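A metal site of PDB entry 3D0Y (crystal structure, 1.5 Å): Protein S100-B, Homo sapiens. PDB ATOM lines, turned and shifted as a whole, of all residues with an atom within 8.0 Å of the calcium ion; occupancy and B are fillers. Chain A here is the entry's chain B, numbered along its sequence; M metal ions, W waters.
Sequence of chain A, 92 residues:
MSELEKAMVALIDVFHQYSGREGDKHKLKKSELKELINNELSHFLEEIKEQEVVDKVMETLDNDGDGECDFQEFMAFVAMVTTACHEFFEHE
The calcium ion is bound by O of Asp 24 (2.2 Å). OE1 of Glu 32 binds the calcium ion (2.3 Å). The calcium ion is bound by O of Lys 27. The calcium ion is bound by O of Ser 19 (2.4 Å). Water W1 binds the calcium ion, 2.5 Å away. The calcium ion is bound by OE2 of Glu 32, 2.5 Å away. O of Glu 22 is bound to the calcium ion, at 2.6 Å.
Water W1 bridges OE2 of Glu 68 (3.0 Å) and NZ of Lys 29 (3.1 Å).
OD1 of Asp 24 sits at hydrogen-bond distance from N of His 26 (2.7 Å). The side-chain hydroxyl (OG) of Ser 19 is in hydrogen-bond range of the backbone carbonyl oxygen (O) of Lys 25. The backbone carbonyl oxygen (O) of Phe 15 is in hydrogen-bond range of the side-chain hydroxyl (OG) of Ser 19 (3.1 Å). The backbone NH (N) of Lys 29 sits close to the side-chain carboxylate (OE1) of Glu 32, at 2.8 Å. The side-chain carboxylate (OE2) of Glu 32 sits close to the backbone NH (N) of Arg 21 (3.3 Å). The side-chain amino group of Lys 27 is in salt-bridge range of the side-chain carboxylate of Asp 24 (2.5 Å).
Within 4 Å of the calcium ion: Ser 19, Glu 22, Asp 24, Lys 27 and Glu 32.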
ATOM      1  N   PHE A  15     -30.639  -7.912  30.451  1.00  0.00           N
ATOM      2  CA  PHE A  15     -29.930  -7.188  29.389  1.00  0.00           C
ATOM      3  C   PHE A  15     -28.584  -6.633  29.866  1.00  0.00           C
ATOM      4  O   PHE A  15     -27.554  -6.880  29.233  1.00  0.00           O
ATOM      5  CB  PHE A  15     -30.785  -6.066  28.750  1.00  0.00           C
ATOM      6  CG  PHE A  15     -30.042  -5.273  27.687  1.00  0.00           C
ATOM      7  CD1 PHE A  15     -29.939  -5.735  26.389  1.00  0.00           C
ATOM      8  CD2 PHE A  15     -29.380  -4.081  28.023  1.00  0.00           C
ATOM      9  CE1 PHE A  15     -29.195  -4.975  25.422  1.00  0.00           C
ATOM     10  CE2 PHE A  15     -28.639  -3.317  27.080  1.00  0.00           C
ATOM     11  CZ  PHE A  15     -28.567  -3.765  25.769  1.00  0.00           C
ATOM     12  N   HIS A  16     -28.617  -5.905  30.991  1.00  0.00           N
ATOM     13  CA  HIS A  16     -27.390  -5.382  31.592  1.00  0.00           C
ATOM     14  C   HIS A  16     -26.419  -6.508  31.967  1.00  0.00           C
ATOM     15  O   HIS A  16     -25.238  -6.392  31.719  1.00  0.00           O
ATOM     16  CB  HIS A  16     -27.752  -4.537  32.813  1.00  0.00           C
ATOM     17  CG  HIS A  16     -28.160  -3.137  32.491  1.00  0.00           C
ATOM     18  ND1 HIS A  16     -29.174  -2.475  33.173  1.00  0.00           N
ATOM     19  CD2 HIS A  16     -27.645  -2.223  31.623  1.00  0.00           C
ATOM     20  CE1 HIS A  16     -29.300  -1.249  32.694  1.00  0.00           C
ATOM     21  NE2 HIS A  16     -28.365  -1.060  31.780  1.00  0.00           N
ATOM     22  N   GLN A  17     -26.925  -7.622  32.511  1.00  0.00           N
ATOM     23  CA  GLN A  17     -26.044  -8.739  32.883  1.00  0.00           C
ATOM     24  C   GLN A  17     -25.132  -9.202  31.724  1.00  0.00           C
ATOM     25  O   GLN A  17     -23.926  -9.469  31.933  1.00  0.00           O
ATOM     26  CB  GLN A  17     -26.837  -9.930  33.415  1.00  0.00           C
ATOM     27  CG  GLN A  17     -27.273  -9.766  34.883  1.00  0.00           C
ATOM     28  CD  GLN A  17     -28.296 -10.815  35.262  1.00  0.00           C
ATOM     29  OE1 GLN A  17     -28.451 -11.819  34.557  1.00  0.00           O
ATOM     30  NE2 GLN A  17     -28.997 -10.597  36.379  1.00  0.00           N
ATOM     31  N   TYR A  18     -25.687  -9.249  30.509  1.00  0.00           N
ATOM     32  CA  TYR A  18     -24.971  -9.781  29.359  1.00  0.00           C
ATOM     33  C   TYR A  18     -24.292  -8.722  28.555  1.00  0.00           C
ATOM     34  O   TYR A  18     -23.150  -8.906  28.070  1.00  0.00           O
ATOM     35  CB  TYR A  18     -25.929 -10.634  28.513  1.00  0.00           C
ATOM     36  CG  TYR A  18     -26.155 -11.961  29.149  1.00  0.00           C
ATOM     37  CD1 TYR A  18     -27.145 -12.141  30.094  1.00  0.00           C
ATOM     38  CD2 TYR A  18     -25.310 -13.022  28.847  1.00  0.00           C
ATOM     39  CE1 TYR A  18     -27.291 -13.344  30.710  1.00  0.00           C
ATOM     40  CE2 TYR A  18     -25.460 -14.213  29.469  1.00  0.00           C
ATOM     41  CZ  TYR A  18     -26.429 -14.380  30.385  1.00  0.00           C
ATOM     42  OH  TYR A  18     -26.554 -15.623  30.947  1.00  0.00           O
ATOM     43  N   SER A  19     -24.935  -7.570  28.490  1.00  0.00           N
ATOM     44  CA  SER A  19     -24.382  -6.472  27.667  1.00  0.00           C
ATOM     45  C   SER A  19     -23.111  -5.927  28.299  1.00  0.00           C
ATOM     46  O   SER A  19     -22.238  -5.360  27.620  1.00  0.00           O
ATOM     47  CB  SER A  19     -25.444  -5.400  27.426  1.00  0.00           C
ATOM     48  OG  SER A  19     -25.582  -4.551  28.571  1.00  0.00           O
ATOM     49  N   GLY A  20     -23.003  -6.105  29.603  1.00  0.00           N
ATOM     50  CA  GLY A  20     -21.910  -5.533  30.369  1.00  0.00           C
ATOM     51  C   GLY A  20     -20.619  -6.311  30.375  1.00  0.00           C
ATOM     52  O   GLY A  20     -19.632  -5.865  30.928  1.00  0.00           O
ATOM     53  N   ARG A  21     -20.589  -7.452  29.705  1.00  0.00           N
ATOM     54  CA  ARG A  21     -19.441  -8.349  29.782  1.00  0.00           C
ATOM     55  C   ARG A  21     -18.220  -7.936  28.976  1.00  0.00           C
ATOM     56  O   ARG A  21     -17.103  -8.021  29.470  1.00  0.00           O
ATOM     57  CB  ARG A  21     -19.854  -9.754  29.361  1.00  0.00           C
ATOM     58  CG  ARG A  21     -20.815 -10.397  30.297  1.00  0.00           C
ATOM     59  CD  ARG A  21     -21.347 -11.622  29.602  1.00  0.00           C
ATOM     60  NE  ARG A  21     -22.005 -12.512  30.534  1.00  0.00           N
ATOM     61  CZ  ARG A  21     -22.205 -13.803  30.315  1.00  0.00           C
ATOM     62  NH1 ARG A  21     -21.812 -14.391  29.187  1.00  0.00           N
ATOM     63  NH2 ARG A  21     -22.803 -14.519  31.230  1.00  0.00           N
ATOM     64  N   GLU A  22     -18.448  -7.506  27.737  1.00  0.00           N
ATOM     65  CA  GLU A  22     -17.385  -7.283  26.766  1.00  0.00           C
ATOM     66  C   GLU A  22     -17.648  -6.007  25.983  1.00  0.00           C
ATOM     67  O   GLU A  22     -18.795  -5.571  25.878  1.00  0.00           O
ATOM     68  CB  GLU A  22     -17.303  -8.456  25.786  1.00  0.00           C
ATOM     69  CG  GLU A  22     -16.710  -9.736  26.361  1.00  0.00           C
ATOM     70  CD  GLU A  22     -16.224 -10.705  25.261  1.00  0.00           C
ATOM     71  OE1 GLU A  22     -15.563 -10.228  24.303  1.00  0.00           O
ATOM     72  OE2 GLU A  22     -16.473 -11.929  25.380  1.00  0.00           O
ATOM     73  N   GLY A  23     -16.580  -5.412  25.443  1.00  0.00           N
ATOM     74  CA  GLY A  23     -16.697  -4.226  24.597  1.00  0.00           C
ATOM     75  C   GLY A  23     -17.620  -3.210  25.216  1.00  0.00           C
ATOM     76  O   GLY A  23     -17.479  -2.968  26.425  1.00  0.00           O
ATOM     77  N   ASP A  24     -18.643  -2.741  24.315  1.00  0.00           N
ATOM     78  CA  ASP A  24     -19.769  -1.891  24.694  1.00  0.00           C
ATOM     79  C   ASP A  24     -20.557  -2.448  25.865  1.00  0.00           C
ATOM     80  O   ASP A  24     -21.227  -3.488  25.706  1.00  0.00           O
ATOM     81  CB  ASP A  24     -20.699  -1.658  23.538  1.00  0.00           C
ATOM     82  CG  ASP A  24     -21.728  -0.594  23.761  1.00  0.00           C
ATOM     83  OD1 ASP A  24     -22.171  -0.402  24.930  1.00  0.00           O
ATOM     84  OD2 ASP A  24     -22.078   0.202  22.732  1.00  0.00           O
ATOM     85  N   LYS A  25     -20.550  -1.731  26.983  1.00  0.00           N
ATOM     86  CA  LYS A  25     -21.142  -2.222  28.233  1.00  0.00           C
ATOM     87  C   LYS A  25     -22.670  -2.161  28.228  1.00  0.00           C
ATOM     88  O   LYS A  25     -23.310  -2.674  29.123  1.00  0.00           O
ATOM     89  CB  LYS A  25     -20.551  -1.440  29.442  1.00  0.00           C
ATOM     90  N   HIS A  26     -23.225  -1.580  27.147  1.00  0.00           N
ATOM     91  CA  HIS A  26     -24.609  -1.215  27.030  1.00  0.00           C
ATOM     92  C   HIS A  26     -25.217  -1.793  25.766  1.00  0.00           C
ATOM     93  O   HIS A  26     -26.334  -1.455  25.387  1.00  0.00           O
ATOM     94  CB  HIS A  26     -24.693   0.305  26.963  1.00  0.00           C
ATOM     95  CG  HIS A  26     -25.779   0.886  27.810  1.00  0.00           C
ATOM     96  ND1 HIS A  26     -26.361   2.116  27.546  1.00  0.00           N
ATOM     97  CD2 HIS A  26     -26.350   0.430  28.954  1.00  0.00           C
ATOM     98  CE1 HIS A  26     -27.257   2.378  28.482  1.00  0.00           C
ATOM     99  NE2 HIS A  26     -27.279   1.365  29.343  1.00  0.00           N
ATOM    100  N   LYS A  27     -24.456  -2.649  25.112  1.00  0.00           N
ATOM    101  CA  LYS A  27     -24.982  -3.387  23.966  1.00  0.00           C
ATOM    102  C   LYS A  27     -24.496  -4.814  24.014  1.00  0.00           C
ATOM    103  O   LYS A  27     -23.461  -5.072  24.638  1.00  0.00           O
ATOM    104  CB  LYS A  27     -24.522  -2.732  22.658  1.00  0.00           C
ATOM    105  CG  LYS A  27     -24.902  -1.295  22.521  1.00  0.00           C
ATOM    106  CD  LYS A  27     -24.733  -0.933  21.093  1.00  0.00           C
ATOM    107  CE  LYS A  27     -25.056   0.515  20.936  1.00  0.00           C
ATOM    108  NZ  LYS A  27     -24.056   1.430  21.699  1.00  0.00           N
ATOM    109  N   LEU A  28     -25.252  -5.717  23.379  1.00  0.00           N
ATOM    110  CA  LEU A  28     -24.931  -7.133  23.250  1.00  0.00           C
ATOM    111  C   LEU A  28     -24.152  -7.381  21.981  1.00  0.00           C
ATOM    112  O   LEU A  28     -24.696  -7.164  20.897  1.00  0.00           O
ATOM    113  CB  LEU A  28     -26.209  -8.031  23.225  1.00  0.00           C
ATOM    114  CG  LEU A  28     -27.115  -7.922  24.421  1.00  0.00           C
ATOM    115  CD1 LEU A  28     -28.399  -8.781  24.237  1.00  0.00           C
ATOM    116  CD2 LEU A  28     -26.386  -8.474  25.608  1.00  0.00           C
ATOM    117  N   LYS A  29     -22.889  -7.809  22.073  1.00  0.00           N
ATOM    118  CA  LYS A  29     -22.216  -8.330  20.874  1.00  0.00           C
ATOM    119  C   LYS A  29     -22.674  -9.756  20.646  1.00  0.00           C
ATOM    120  O   LYS A  29     -23.414 -10.315  21.478  1.00  0.00           O
ATOM    121  CB  LYS A  29     -20.685  -8.213  20.934  1.00  0.00           C
ATOM    122  CG  LYS A  29     -20.021  -8.780  22.161  1.00  0.00           C
ATOM    123  CD  LYS A  29     -18.504  -8.915  21.984  1.00  0.00           C
ATOM    124  CE  LYS A  29     -17.826  -7.713  21.285  1.00  0.00           C
ATOM    125  NZ  LYS A  29     -17.814  -6.422  22.072  1.00  0.00           N
ATOM    126  N   LYS A  30     -22.249 -10.358  19.531  1.00  0.00           N
ATOM    127  CA  LYS A  30     -22.670 -11.739  19.234  1.00  0.00           C
ATOM    128  C   LYS A  30     -22.435 -12.750  20.363  1.00  0.00           C
ATOM    129  O   LYS A  30     -23.334 -13.544  20.684  1.00  0.00           O
ATOM    130  CB  LYS A  30     -22.033 -12.234  17.949  1.00  0.00           C
ATOM    131  CG  LYS A  30     -22.535 -11.526  16.716  1.00  0.00           C
ATOM    132  CD  LYS A  30     -21.993 -12.240  15.484  1.00  0.00           C
ATOM    133  CE  LYS A  30     -21.909 -11.319  14.295  1.00  0.00           C
ATOM    134  NZ  LYS A  30     -21.329 -12.037  13.159  1.00  0.00           N
ATOM    135  N   GLU A  32     -22.153 -12.201  23.551  1.00  0.00           N
ATOM    136  CA  GLU A  32     -23.028 -11.907  24.692  1.00  0.00           C
ATOM    137  C   GLU A  32     -24.477 -12.333  24.385  1.00  0.00           C
ATOM    138  O   GLU A  32     -25.168 -12.838  25.253  1.00  0.00           O
ATOM    139  CB  GLU A  32     -22.982 -10.413  25.020  1.00  0.00           C
ATOM    140  CG  GLU A  32     -21.632  -9.921  25.543  1.00  0.00           C
ATOM    141  CD  GLU A  32     -21.523  -8.394  25.604  1.00  0.00           C
ATOM    142  OE1 GLU A  32     -22.213  -7.674  24.801  1.00  0.00           O
ATOM    143  OE2 GLU A  32     -20.729  -7.902  26.436  1.00  0.00           O
ATOM    144  N   LEU A  33     -24.929 -12.062  23.167  1.00  0.00           N
ATOM    145  CA  LEU A  33     -26.245 -12.480  22.712  1.00  0.00           C
ATOM    146  C   LEU A  33     -26.407 -14.024  22.735  1.00  0.00           C
ATOM    147  O   LEU A  33     -27.451 -14.509  23.172  1.00  0.00           O
ATOM    148  CB  LEU A  33     -26.527 -11.903  21.314  1.00  0.00           C
ATOM    149  CG  LEU A  33     -27.878 -12.277  20.704  1.00  0.00           C
ATOM    150  CD1 LEU A  33     -29.057 -11.808  21.589  1.00  0.00           C
ATOM    151  CD2 LEU A  33     -27.983 -11.727  19.283  1.00  0.00           C
ATOM    152  N   GLU A  68     -24.246  -4.970  16.790  1.00  0.00           N
ATOM    153  CA  GLU A  68     -24.647  -5.238  18.175  1.00  0.00           C
ATOM    154  C   GLU A  68     -26.154  -5.116  18.367  1.00  0.00           C
ATOM    155  O   GLU A  68     -26.871  -4.597  17.510  1.00  0.00           O
ATOM    156  CB  GLU A  68     -23.893  -4.382  19.189  1.00  0.00           C
ATOM    157  CG  GLU A  68     -22.363  -4.429  19.022  1.00  0.00           C
ATOM    158  CD  GLU A  68     -21.581  -4.416  20.353  1.00  0.00           C
ATOM    159  OE1 GLU A  68     -22.171  -4.603  21.441  1.00  0.00           O
ATOM    160  OE2 GLU A  68     -20.349  -4.236  20.280  1.00  0.00           O
ATOM    161  N   CYS A  69     -26.611  -5.642  19.503  1.00  0.00           N
ATOM    162  CA  CYS A  69     -27.996  -5.551  19.920  1.00  0.00           C
ATOM    163  C   CYS A  69     -28.073  -4.574  21.093  1.00  0.00           C
ATOM    164  O   CYS A  69     -27.544  -4.852  22.191  1.00  0.00           O
ATOM    165  CB  CYS A  69     -28.514  -6.915  20.385  1.00  0.00           C
ATOM    166  SG  CYS A  69     -30.278  -6.847  20.777  1.00  0.00           S
HETATM  167 CA    CA M   1     -21.315  -5.701  25.414  1.00  0.00          CA
HETATM  168  O   HOH W   1     -20.603  -5.390  23.062  1.00  0.00           O
